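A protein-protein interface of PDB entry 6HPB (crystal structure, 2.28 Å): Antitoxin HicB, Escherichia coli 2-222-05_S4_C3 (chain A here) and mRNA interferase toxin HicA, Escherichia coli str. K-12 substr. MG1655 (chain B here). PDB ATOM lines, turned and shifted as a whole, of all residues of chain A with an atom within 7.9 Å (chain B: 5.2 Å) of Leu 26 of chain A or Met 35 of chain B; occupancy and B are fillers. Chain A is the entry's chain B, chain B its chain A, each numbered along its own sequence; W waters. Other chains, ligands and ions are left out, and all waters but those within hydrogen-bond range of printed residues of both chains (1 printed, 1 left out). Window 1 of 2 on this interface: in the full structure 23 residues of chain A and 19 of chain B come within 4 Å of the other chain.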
ATOM      1  N   MET A  16      24.311  10.436  18.265  1.00  0.00           N
ATOM      2  CA  MET A  16      23.411  11.222  17.454  1.00  0.00           C
ATOM      3  C   MET A  16      24.250  12.290  16.772  1.00  0.00           C
ATOM      4  O   MET A  16      25.175  12.836  17.384  1.00  0.00           O
ATOM      5  CB  MET A  16      22.309  11.884  18.270  1.00  0.00           C
ATOM      6  CG  MET A  16      21.501  12.844  17.420  1.00  0.00           C
ATOM      7  SD  MET A  16      20.460  14.133  18.383  1.00  0.00           S
ATOM      8  CE  MET A  16      21.815  15.076  19.392  1.00  0.00           C
ATOM      9  N   VAL A  17      23.925  12.576  15.516  1.00  0.00           N
ATOM     10  CA  VAL A  17      24.605  13.584  14.716  1.00  0.00           C
ATOM     11  C   VAL A  17      23.668  14.764  14.500  1.00  0.00           C
ATOM     12  O   VAL A  17      22.510  14.579  14.114  1.00  0.00           O
ATOM     13  CB  VAL A  17      25.060  13.001  13.373  1.00  0.00           C
ATOM     14  CG1 VAL A  17      25.748  14.081  12.527  1.00  0.00           C
ATOM     15  CG2 VAL A  17      25.961  11.839  13.610  1.00  0.00           C
ATOM     16  N   SER A  18      24.145  15.964  14.789  1.00  0.00           N
ATOM     17  CA  SER A  18      23.396  17.181  14.503  1.00  0.00           C
ATOM     18  C   SER A  18      24.326  18.204  13.858  1.00  0.00           C
ATOM     19  O   SER A  18      25.550  18.066  13.886  1.00  0.00           O
ATOM     20  CB  SER A  18      22.741  17.752  15.749  1.00  0.00           C
ATOM     21  OG  SER A  18      23.719  18.026  16.723  1.00  0.00           O
ATOM     22  N   PHE A  19      23.732  19.237  13.260  1.00  0.00           N
ATOM     23  CA  PHE A  19      24.484  20.315  12.627  1.00  0.00           C
ATOM     24  C   PHE A  19      23.948  21.660  13.096  1.00  0.00           C
ATOM     25  O   PHE A  19      22.780  21.990  12.854  1.00  0.00           O
ATOM     26  CB  PHE A  19      24.365  20.236  11.103  1.00  0.00           C
ATOM     27  CG  PHE A  19      25.148  19.122  10.461  1.00  0.00           C
ATOM     28  CD1 PHE A  19      24.664  17.836  10.464  1.00  0.00           C
ATOM     29  CD2 PHE A  19      26.337  19.394   9.798  1.00  0.00           C
ATOM     30  CE1 PHE A  19      25.362  16.828   9.834  1.00  0.00           C
ATOM     31  CE2 PHE A  19      27.041  18.411   9.166  1.00  0.00           C
ATOM     32  CZ  PHE A  19      26.570  17.114   9.199  1.00  0.00           C
ATOM     33  N   ILE A  22      22.536  23.629  10.037  1.00  0.00           N
ATOM     34  CA  ILE A  22      21.526  23.001   9.190  1.00  0.00           C
ATOM     35  C   ILE A  22      20.566  22.215  10.075  1.00  0.00           C
ATOM     36  O   ILE A  22      20.862  21.062  10.422  1.00  0.00           O
ATOM     37  CB  ILE A  22      22.200  22.107   8.140  1.00  0.00           C
ATOM     38  CG1 ILE A  22      23.168  22.924   7.289  1.00  0.00           C
ATOM     39  CG2 ILE A  22      21.156  21.365   7.276  1.00  0.00           C
ATOM     40  CD1 ILE A  22      22.478  24.074   6.543  1.00  0.00           C
ATOM     41  N   PRO A  23      19.398  22.769  10.432  1.00  0.00           N
ATOM     42  CA  PRO A  23      18.545  22.092  11.427  1.00  0.00           C
ATOM     43  C   PRO A  23      17.966  20.772  10.939  1.00  0.00           C
ATOM     44  O   PRO A  23      17.612  19.929  11.765  1.00  0.00           O
ATOM     45  CB  PRO A  23      17.448  23.120  11.711  1.00  0.00           C
ATOM     46  CG  PRO A  23      17.919  24.412  11.086  1.00  0.00           C
ATOM     47  CD  PRO A  23      18.789  24.022   9.956  1.00  0.00           C
ATOM     48  N   GLU A  24      17.809  20.598   9.628  1.00  0.00           N
ATOM     49  CA  GLU A  24      17.260  19.380   9.039  1.00  0.00           C
ATOM     50  C   GLU A  24      18.194  18.186   9.116  1.00  0.00           C
ATOM     51  O   GLU A  24      17.722  17.055   8.987  1.00  0.00           O
ATOM     52  CB  GLU A  24      16.917  19.617   7.554  1.00  0.00           C
ATOM     53  CG  GLU A  24      15.801  20.641   7.354  1.00  0.00           C
ATOM     54  CD  GLU A  24      16.315  22.055   7.363  1.00  0.00           C
ATOM     55  OE1 GLU A  24      17.541  22.245   7.463  1.00  0.00           O
ATOM     56  OE2 GLU A  24      15.498  22.983   7.318  1.00  0.00           O
ATOM     57  N   ALA A  25      19.496  18.398   9.278  1.00  0.00           N
ATOM     58  CA  ALA A  25      20.472  17.311   9.148  1.00  0.00           C
ATOM     59  C   ALA A  25      20.604  16.588  10.492  1.00  0.00           C
ATOM     60  O   ALA A  25      21.347  17.009  11.380  1.00  0.00           O
ATOM     61  CB  ALA A  25      21.802  17.875   8.660  1.00  0.00           C
ATOM     62  N   LEU A  26      19.906  15.477  10.633  1.00  0.00           N
ATOM     63  CA  LEU A  26      19.810  14.772  11.904  1.00  0.00           C
ATOM     64  C   LEU A  26      19.960  13.298  11.593  1.00  0.00           C
ATOM     65  O   LEU A  26      19.240  12.781  10.730  1.00  0.00           O
ATOM     66  CB  LEU A  26      18.478  15.047  12.607  1.00  0.00           C
ATOM     67  CG  LEU A  26      18.172  16.489  13.015  1.00  0.00           C
ATOM     68  CD1 LEU A  26      16.709  16.657  13.402  1.00  0.00           C
ATOM     69  CD2 LEU A  26      19.060  16.901  14.173  1.00  0.00           C
ATOM     70  N   THR A  27      20.916  12.641  12.244  1.00  0.00           N
ATOM     71  CA  THR A  27      21.146  11.225  11.964  1.00  0.00           C
ATOM     72  C   THR A  27      21.916  10.600  13.127  1.00  0.00           C
ATOM     73  O   THR A  27      22.039  11.204  14.198  1.00  0.00           O
ATOM     74  CB  THR A  27      21.860  11.061  10.618  1.00  0.00           C
ATOM     75  OG1 THR A  27      21.974   9.666  10.304  1.00  0.00           O
ATOM     76  CG2 THR A  27      23.234  11.732  10.641  1.00  0.00           C
ATOM     77  N   GLN A  28      22.455   9.391  12.919  1.00  0.00           N
ATOM     78  CA  GLN A  28      23.137   8.704  14.018  1.00  0.00           C
ATOM     79  C   GLN A  28      24.197   7.746  13.486  1.00  0.00           C
ATOM     80  O   GLN A  28      24.355   7.561  12.280  1.00  0.00           O
ATOM     81  CB  GLN A  28      22.130   7.915  14.862  1.00  0.00           C
ATOM     82  CG  GLN A  28      21.503   6.728  14.110  1.00  0.00           C
ATOM     83  CD  GLN A  28      20.446   5.985  14.915  1.00  0.00           C
ATOM     84  OE1 GLN A  28      19.631   6.598  15.587  1.00  0.00           O
ATOM     85  NE2 GLN A  28      20.439   4.660  14.824  1.00  0.00           N
ATOM     86  N   ALA A  38      27.537   8.984   8.103  1.00  0.00           N
ATOM     87  CA  ALA A  38      26.142   9.370   8.087  1.00  0.00           C
ATOM     88  C   ALA A  38      26.015  10.886   8.099  1.00  0.00           C
ATOM     89  O   ALA A  38      25.124  11.444   7.451  1.00  0.00           O
ATOM     90  CB  ALA A  38      25.419   8.760   9.292  1.00  0.00           C
ATOM     91  N   ALA A  39      26.928  11.566   8.792  1.00  0.00           N
ATOM     92  CA  ALA A  39      26.858  13.015   8.870  1.00  0.00           C
ATOM     93  C   ALA A  39      26.936  13.636   7.482  1.00  0.00           C
ATOM     94  O   ALA A  39      26.172  14.553   7.163  1.00  0.00           O
ATOM     95  CB  ALA A  39      27.971  13.553   9.758  1.00  0.00           C
ATOM     96  N   ASP A  41      26.239  12.226   4.436  1.00  0.00           N
ATOM     97  CA  ASP A  41      25.026  11.875   3.699  1.00  0.00           C
ATOM     98  C   ASP A  41      23.834  12.684   4.197  1.00  0.00           C
ATOM     99  O   ASP A  41      23.009  13.157   3.402  1.00  0.00           O
ATOM    100  CB  ASP A  41      24.763  10.375   3.861  1.00  0.00           C
ATOM    101  CG  ASP A  41      23.762   9.813   2.855  1.00  0.00           C
ATOM    102  OD1 ASP A  41      22.564  10.147   2.879  1.00  0.00           O
ATOM    103  OD2 ASP A  41      24.183   8.954   2.070  1.00  0.00           O
ATOM    104  N   ALA A  42      23.722  12.852   5.515  1.00  0.00           N
ATOM    105  CA  ALA A  42      22.597  13.610   6.062  1.00  0.00           C
ATOM    106  C   ALA A  42      22.701  15.090   5.706  1.00  0.00           C
ATOM    107  O   ALA A  42      21.682  15.745   5.444  1.00  0.00           O
ATOM    108  CB  ALA A  42      22.504  13.421   7.574  1.00  0.00           C
ATOM    109  N   LEU A  43      23.910  15.648   5.731  1.00  0.00           N
ATOM    110  CA  LEU A  43      24.045  17.047   5.361  1.00  0.00           C
ATOM    111  C   LEU A  43      23.715  17.246   3.870  1.00  0.00           C
ATOM    112  O   LEU A  43      22.875  18.084   3.518  1.00  0.00           O
ATOM    113  CB  LEU A  43      25.459  17.521   5.682  1.00  0.00           C
ATOM    114  CG  LEU A  43      25.833  18.926   5.236  1.00  0.00           C
ATOM    115  CD1 LEU A  43      25.060  19.948   6.037  1.00  0.00           C
ATOM    116  CD2 LEU A  43      27.311  19.176   5.368  1.00  0.00           C
ATOM    117  N   THR A  45      21.972  15.342   1.921  1.00  0.00           N
ATOM    118  CA  THR A  45      20.544  15.111   1.703  1.00  0.00           C
ATOM    119  C   THR A  45      19.719  16.329   2.096  1.00  0.00           C
ATOM    120  O   THR A  45      18.819  16.738   1.356  1.00  0.00           O
ATOM    121  CB  THR A  45      20.072  13.874   2.456  1.00  0.00           C
ATOM    122  OG1 THR A  45      20.855  12.744   2.042  1.00  0.00           O
ATOM    123  CG2 THR A  45      18.610  13.601   2.140  1.00  0.00           C
ATOM    124  N   ALA A  46      20.017  16.925   3.257  1.00  0.00           N
ATOM    125  CA  ALA A  46      19.258  18.080   3.714  1.00  0.00           C
ATOM    126  C   ALA A  46      19.349  19.248   2.731  1.00  0.00           C
ATOM    127  O   ALA A  46      18.407  20.038   2.613  1.00  0.00           O
ATOM    128  CB  ALA A  46      19.761  18.510   5.090  1.00  0.00           C
ATOM    129  N   PHE A  49      16.363  19.979   0.379  1.00  0.00           N
ATOM    130  CA  PHE A  49      15.203  20.745   0.821  1.00  0.00           C
ATOM    131  C   PHE A  49      15.310  22.188   0.356  1.00  0.00           C
ATOM    132  O   PHE A  49      14.315  22.806  -0.029  1.00  0.00           O
ATOM    133  CB  PHE A  49      15.083  20.742   2.337  1.00  0.00           C
ATOM    134  CG  PHE A  49      14.645  19.425   2.954  1.00  0.00           C
ATOM    135  CD1 PHE A  49      13.426  18.849   2.649  1.00  0.00           C
ATOM    136  CD2 PHE A  49      15.445  18.813   3.900  1.00  0.00           C
ATOM    137  CE1 PHE A  49      13.030  17.647   3.241  1.00  0.00           C
ATOM    138  CE2 PHE A  49      15.048  17.617   4.518  1.00  0.00           C
ATOM    139  CZ  PHE A  49      13.837  17.042   4.191  1.00  0.00           C
ATOM    140  N   GLN B   3      13.735   1.788  13.614  1.00  0.00           N
ATOM    141  CA  GLN B   3      13.550   2.894  12.667  1.00  0.00           C
ATOM    142  C   GLN B   3      12.372   2.639  11.741  1.00  0.00           C
ATOM    143  O   GLN B   3      11.629   3.569  11.403  1.00  0.00           O
ATOM    144  CB  GLN B   3      14.823   3.135  11.866  1.00  0.00           C
ATOM    145  CG  GLN B   3      15.734   4.134  12.585  1.00  0.00           C
ATOM    146  CD  GLN B   3      16.970   4.524  11.797  1.00  0.00           C
ATOM    147  OE1 GLN B   3      16.941   4.617  10.572  1.00  0.00           O
ATOM    148  NE2 GLN B   3      18.079   4.734  12.510  1.00  0.00           N
ATOM    149  N   PHE B   6       9.332   3.619  13.668  1.00  0.00           N
ATOM    150  CA  PHE B   6       9.339   5.061  13.862  1.00  0.00           C
ATOM    151  C   PHE B   6       8.871   5.787  12.604  1.00  0.00           C
ATOM    152  O   PHE B   6       8.095   6.752  12.686  1.00  0.00           O
ATOM    153  CB  PHE B   6      10.733   5.542  14.263  1.00  0.00           C
ATOM    154  CG  PHE B   6      10.804   7.017  14.513  1.00  0.00           C
ATOM    155  CD1 PHE B   6      10.002   7.607  15.471  1.00  0.00           C
ATOM    156  CD2 PHE B   6      11.660   7.817  13.782  1.00  0.00           C
ATOM    157  CE1 PHE B   6      10.063   8.965  15.712  1.00  0.00           C
ATOM    158  CE2 PHE B   6      11.724   9.173  14.019  1.00  0.00           C
ATOM    159  CZ  PHE B   6      10.921   9.749  14.983  1.00  0.00           C
ATOM    160  N   ARG B   7       9.307   5.314  11.427  1.00  0.00           N
ATOM    161  CA  ARG B   7       8.835   5.913  10.185  1.00  0.00           C
ATOM    162  C   ARG B   7       7.373   5.576   9.927  1.00  0.00           C
ATOM    163  O   ARG B   7       6.625   6.428   9.442  1.00  0.00           O
ATOM    164  CB  ARG B   7       9.684   5.433   9.005  1.00  0.00           C
ATOM    165  CG  ARG B   7       8.848   5.170   7.752  1.00  0.00           C
ATOM    166  CD  ARG B   7       9.623   4.677   6.561  1.00  0.00           C
ATOM    167  NE  ARG B   7       8.837   4.892   5.351  1.00  0.00           N
ATOM    168  CZ  ARG B   7       9.309   4.829   4.105  1.00  0.00           C
ATOM    169  NH1 ARG B   7      10.587   4.526   3.874  1.00  0.00           N
ATOM    170  NH2 ARG B   7       8.489   5.061   3.083  1.00  0.00           N
ATOM    171  N   LEU B  10       5.648   8.094  12.012  1.00  0.00           N
ATOM    172  CA  LEU B  10       5.716   9.373  11.302  1.00  0.00           C
ATOM    173  C   LEU B  10       4.638   9.434  10.230  1.00  0.00           C
ATOM    174  O   LEU B  10       3.874  10.404  10.134  1.00  0.00           O
ATOM    175  CB  LEU B  10       7.095   9.553  10.668  1.00  0.00           C
ATOM    176  CG  LEU B  10       8.107  10.473  11.344  1.00  0.00           C
ATOM    177  CD1 LEU B  10       7.657  10.861  12.727  1.00  0.00           C
ATOM    178  CD2 LEU B  10       9.493   9.843  11.352  1.00  0.00           C
ATOM    179  N   HIS B  23      19.602   9.741   2.863  1.00  0.00           N
ATOM    180  CA  HIS B  23      18.746   9.809   4.025  1.00  0.00           C
ATOM    181  C   HIS B  23      17.318  10.073   3.577  1.00  0.00           C
ATOM    182  O   HIS B  23      17.072  10.673   2.522  1.00  0.00           O
ATOM    183  CB  HIS B  23      19.215  10.903   4.977  1.00  0.00           C
ATOM    184  CG  HIS B  23      20.263  10.449   5.939  1.00  0.00           C
ATOM    185  ND1 HIS B  23      21.505  10.015   5.527  1.00  0.00           N
ATOM    186  CD2 HIS B  23      20.259  10.360   7.290  1.00  0.00           C
ATOM    187  CE1 HIS B  23      22.227   9.690   6.582  1.00  0.00           C
ATOM    188  NE2 HIS B  23      21.493   9.882   7.664  1.00  0.00           N
ATOM    189  N   LEU B  24      16.376   9.580   4.370  1.00  0.00           N
ATOM    190  CA  LEU B  24      14.977   9.843   4.102  1.00  0.00           C
ATOM    191  C   LEU B  24      14.680  11.319   4.346  1.00  0.00           C
ATOM    192  O   LEU B  24      15.225  11.926   5.265  1.00  0.00           O
ATOM    193  CB  LEU B  24      14.099   8.975   4.993  1.00  0.00           C
ATOM    194  CG  LEU B  24      14.089   7.463   4.725  1.00  0.00           C
ATOM    195  CD1 LEU B  24      13.182   6.691   5.710  1.00  0.00           C
ATOM    196  CD2 LEU B  24      13.628   7.208   3.320  1.00  0.00           C
ATOM    197  N   LEU B  26      11.876  14.026   5.273  1.00  0.00           N
ATOM    198  CA  LEU B  26      10.593  14.129   5.969  1.00  0.00           C
ATOM    199  C   LEU B  26      10.053  15.554   5.906  1.00  0.00           C
ATOM    200  O   LEU B  26      10.799  16.517   6.123  1.00  0.00           O
ATOM    201  CB  LEU B  26      10.734  13.698   7.432  1.00  0.00           C
ATOM    202  CG  LEU B  26      11.443  12.348   7.610  1.00  0.00           C
ATOM    203  CD1 LEU B  26      11.894  12.163   9.041  1.00  0.00           C
ATOM    204  CD2 LEU B  26      10.567  11.177   7.169  1.00  0.00           C
ATOM    205  N   SER B  33      12.894  17.551   7.828  1.00  0.00           N
ATOM    206  CA  SER B  33      13.982  16.892   8.527  1.00  0.00           C
ATOM    207  C   SER B  33      14.400  15.699   7.693  1.00  0.00           C
ATOM    208  O   SER B  33      13.595  15.161   6.927  1.00  0.00           O
ATOM    209  CB  SER B  33      13.540  16.418   9.922  1.00  0.00           C
ATOM    210  OG  SER B  33      14.538  15.618  10.521  1.00  0.00           O
ATOM    211  N   VAL B  34      15.641  15.261   7.874  1.00  0.00           N
ATOM    212  CA  VAL B  34      16.077  14.005   7.307  1.00  0.00           C
ATOM    213  C   VAL B  34      16.119  12.970   8.432  1.00  0.00           C
ATOM    214  O   VAL B  34      15.887  13.279   9.596  1.00  0.00           O
ATOM    215  CB  VAL B  34      17.456  14.098   6.579  1.00  0.00           C
ATOM    216  CG1 VAL B  34      17.551  15.322   5.715  1.00  0.00           C
ATOM    217  CG2 VAL B  34      18.624  14.058   7.554  1.00  0.00           C
ATOM    218  N   MET B  35      16.444  11.737   8.069  1.00  0.00           N
ATOM    219  CA  MET B  35      16.380  10.597   8.958  1.00  0.00           C
ATOM    220  C   MET B  35      17.122   9.466   8.241  1.00  0.00           C
ATOM    221  O   MET B  35      17.004   9.349   7.030  1.00  0.00           O
ATOM    222  CB  MET B  35      14.924  10.250   9.214  1.00  0.00           C
ATOM    223  CG  MET B  35      14.657   9.137  10.165  1.00  0.00           C
ATOM    224  SD  MET B  35      12.850   8.440   9.935  1.00  0.00           S
ATOM    225  CE  MET B  35      13.316   6.609  10.470  1.00  0.00           C
ATOM    226  N   PRO B  36      17.900   8.652   8.958  1.00  0.00           N
ATOM    227  CA  PRO B  36      18.647   7.587   8.274  1.00  0.00           C
ATOM    228  C   PRO B  36      17.691   6.632   7.575  1.00  0.00           C
ATOM    229  O   PRO B  36      16.498   6.577   7.890  1.00  0.00           O
ATOM    230  CB  PRO B  36      19.433   6.899   9.401  1.00  0.00           C
ATOM    231  CG  PRO B  36      18.893   7.431  10.662  1.00  0.00           C
ATOM    232  CD  PRO B  36      18.193   8.718  10.400  1.00  0.00           C
ATOM    233  N   ARG B  37      18.204   5.983   6.527  1.00  0.00           N
ATOM    234  CA  ARG B  37      17.468   4.956   5.798  1.00  0.00           C
ATOM    235  C   ARG B  37      18.005   3.584   6.189  1.00  0.00           C
ATOM    236  O   ARG B  37      18.656   2.885   5.420  1.00  0.00           O
ATOM    237  CB  ARG B  37      17.540   5.205   4.278  1.00  0.00           C
ATOM    238  CG  ARG B  37      16.821   4.163   3.406  1.00  0.00           C
ATOM    239  CD  ARG B  37      17.230   4.250   1.926  1.00  0.00           C
ATOM    240  NE  ARG B  37      16.937   5.586   1.417  1.00  0.00           N
ATOM    241  CZ  ARG B  37      15.717   5.993   1.093  1.00  0.00           C
ATOM    242  NH1 ARG B  37      14.695   5.157   1.202  1.00  0.00           N
ATOM    243  NH2 ARG B  37      15.508   7.229   0.670  1.00  0.00           N
ATOM    244  N   ILE B  43      16.379   3.370  16.256  1.00  0.00           N
ATOM    245  CA  ILE B  43      16.474   4.822  16.307  1.00  0.00           C
ATOM    246  C   ILE B  43      16.895   5.214  17.720  1.00  0.00           C
ATOM    247  O   ILE B  43      16.227   4.879  18.698  1.00  0.00           O
ATOM    248  CB  ILE B  43      15.169   5.514  15.886  1.00  0.00           C
ATOM    249  CG1 ILE B  43      15.353   7.033  16.037  1.00  0.00           C
ATOM    250  CG2 ILE B  43      13.974   5.031  16.706  1.00  0.00           C
ATOM    251  CD1 ILE B  43      14.742   7.841  14.986  1.00  0.00           C
ATOM    252  N   LEU B  47      18.109  11.101  18.937  1.00  0.00           N
ATOM    253  CA  LEU B  47      17.764  11.315  17.519  1.00  0.00           C
ATOM    254  C   LEU B  47      16.262  11.353  17.320  1.00  0.00           C
ATOM    255  O   LEU B  47      15.739  12.270  16.688  1.00  0.00           O
ATOM    256  CB  LEU B  47      18.363  10.234  16.632  1.00  0.00           C
ATOM    257  CG  LEU B  47      18.069  10.340  15.128  1.00  0.00           C
ATOM    258  CD1 LEU B  47      18.223  11.754  14.600  1.00  0.00           C
ATOM    259  CD2 LEU B  47      18.983   9.417  14.367  1.00  0.00           C
ATOM    260  N   ALA B  50      15.084  14.609  18.613  1.00  0.00           N
ATOM    261  CA  ALA B  50      15.471  15.738  17.773  1.00  0.00           C
ATOM    262  C   ALA B  50      14.585  15.835  16.531  1.00  0.00           C
ATOM    263  O   ALA B  50      14.162  16.934  16.156  1.00  0.00           O
ATOM    264  CB  ALA B  50      16.947  15.651  17.388  1.00  0.00           C
ATOM    265  N   ILE B  51      14.229  14.695  15.933  1.00  0.00           N
ATOM    266  CA  ILE B  51      13.398  14.696  14.723  1.00  0.00           C
ATOM    267  C   ILE B  51      11.988  15.197  15.037  1.00  0.00           C
ATOM    268  O   ILE B  51      11.454  16.079  14.349  1.00  0.00           O
ATOM    269  CB  ILE B  51      13.381  13.295  14.081  1.00  0.00           C
ATOM    270  CG1 ILE B  51      14.775  12.923  13.589  1.00  0.00           C
ATOM    271  CG2 ILE B  51      12.468  13.255  12.901  1.00  0.00           C
ATOM    272  CD1 ILE B  51      14.852  11.555  12.990  1.00  0.00           C
ATOM    273  N   GLN B  54      12.178  18.818  15.447  1.00  0.00           N
ATOM    274  CA  GLN B  54      12.416  19.475  14.176  1.00  0.00           C
ATOM    275  C   GLN B  54      11.164  19.493  13.321  1.00  0.00           C
ATOM    276  O   GLN B  54      10.910  20.475  12.615  1.00  0.00           O
ATOM    277  CB  GLN B  54      13.551  18.763  13.454  1.00  0.00           C
ATOM    278  CG  GLN B  54      13.790  19.252  12.057  1.00  0.00           C
ATOM    279  CD  GLN B  54      14.040  20.752  12.002  1.00  0.00           C
ATOM    280  OE1 GLN B  54      14.563  21.350  12.946  1.00  0.00           O
ATOM    281  NE2 GLN B  54      13.699  21.354  10.879  1.00  0.00           N
HETATM  282  O   HOH W   1      17.258  20.230  14.493  1.00  0.00           O
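The side-chain amide nitrogen (NE2) of Gln 3 of chain B lies close to the side-chain amide nitrogen (NE2) of Gln 28 of chain A, 3.3 Å away.
A ring nitrogen (NE2) of His 23 of chain B lies within hydrogen-bond range of the side-chain hydroxyl (OG1) of Thr 27 of chain A (2.7 Å).
OD1 of Asp 41 of chain A is in hydrogen-bond range of ND1 of His 23 of chain B (2.9 Å).
N of His 23 of chain B lies within hydrogen-bond range of OG1 of Thr 45 of chain A (3.4 Å).
The backbone NH (N) of Val 34 of chain B lies within hydrogen-bond range of the backbone carbonyl oxygen (O) of Glu 24 of chain A, 3.0 Å away.
Water W1 bridges O of Pro 23 of chain A and OE1 of Gln 54 of chain B.
Among the printed residues, merely in contact across the chains: Gln 28 of chain A with Leu 47 of chain B (3.1 Å), Phe 49 of chain A with Ser 33 of chain B (3.3 Å), Thr 27 of chain A with Leu 47 of chain B (3.4 Å), Leu 26 of chain A with Val 34 of chain B (3.5 Å), Ala 38 of chain A with His 23 of chain B (3.5 Å), Pro 23 of chain A with Gln 54 of chain B (3.6 Å), Ala 42 of chain A with His 23 of chain B (3.6 Å), Phe 49 of chain A with Val 34 of chain B (3.6 Å), Phe 49 of chain A with Leu 26 of chain B (3.6 Å), Gln 28 of chain A with Ile 43 of chain B (3.7 Å), Leu 26 of chain A with Ser 33 of chain B (3.8 Å), Leu 26 of chain A with Ala 50 of chain B (3.8 Å), Glu 24 of chain A with Ser 33 of chain B (3.8 Å), Leu 26 of chain A with Gln 54 of chain B (3.8 Å), Leu 26 of chain A with Leu 47 of chain B (3.8 Å), Ala 46 of chain A with Val 34 of chain B (3.8 Å), Thr 27 of chain A with Pro 36 of chain B (3.8 Å), Met 16 of chain A with Leu 47 of chain B (3.9 Å), Ala 42 of chain A with Val 34 of chain B (3.9 Å), Met 16 of chain A with Ala 50 of chain B (3.95 Å) and Leu 26 of chain A with Met 35 of chain B (3.999 Å).
The side-chain amide oxygen of Gln 3 of chain B sits close to the backbone carbonyl oxygen of Pro 36 of chain B.
The backbone NH (N) of Leu 24 of chain B lies within hydrogen-bond range of the backbone carbonyl oxygen (O) of Met 35 of chain B (2.7 Å).
N of Leu 26 of chain B sits at hydrogen-bond distance from O of Ser 33 of chain B.
The backbone carbonyl oxygen (O) of Thr 27 of chain A is in hydrogen-bond range of the backbone NH (N) of Val 17 of chain A (2.7 Å).
The side-chain hydroxyl of Thr 45 of chain A sits at hydrogen-bond distance from the backbone carbonyl oxygen of Asp 41 of chain A (2.6 Å).
Of the 19 printed residues of chain A, 12 touch a printed residue of chain B.
Hydrophobic or aromatic side chains of chain A that line the printed part of chain B: Met 16, Pro 23, Leu 26, Ala 42, Ala 46 and Phe 49.
Of the 17 printed residues of chain B, 11 touch a printed residue of chain A.
Hydrophobic or aromatic side chains of chain B that line the printed part of chain A: His 23, Val 34, Pro 36, Leu 47 and Ala 50.
Among the printed residues, 26 pairs touch across the chains.
Among the printed residues, no Asp or Glu carboxylate lies within 4 Å of a Lys or Arg side-chain nitrogen of the other chain.
Of the printed residues of chain B, Leu 26 of chain A touches Ser 33, Val 34, Met 35, Leu 47, Ala 50 and Gln 54.
Printed residues of chain A within 4 Å of Met 35 of chain B: Leu 26 (3.999 Å).
Of chain A, only Thr 27 (3.8 Å) comes within 4 Å of Pro 36 of chain B.
Printed residues of chain A within 4 Å of Leu 47 of chain B: Met 16 (3.9 Å), Leu 26 (3.8 Å), Thr 27 (3.4 Å) and Gln 28 (3.1 Å).
Of the printed residues of chain A, His 23 of chain B touches Thr 27, Ala 38, Asp 41, Ala 42 and Thr 45.
Of the printed residues of chain A, Gln 3 of chain B touches Gln 28.
Of the printed residues of chain B, Ala 42 of chain A touches His 23 (3.6 Å) and Val 34 (3.9 Å).
Printed residues of chain B within 4 Å of Pro 23 of chain A: Gln 54 (3.6 Å).
Ile 22 of chain A touches none of the printed residues of chain B.
Ala 39 of chain A touches none of the printed residues of chain B.
The nearest printed residue of chain A that does not touch Gln 54 of chain B is Glu 24 of chain A (4.2 Å).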
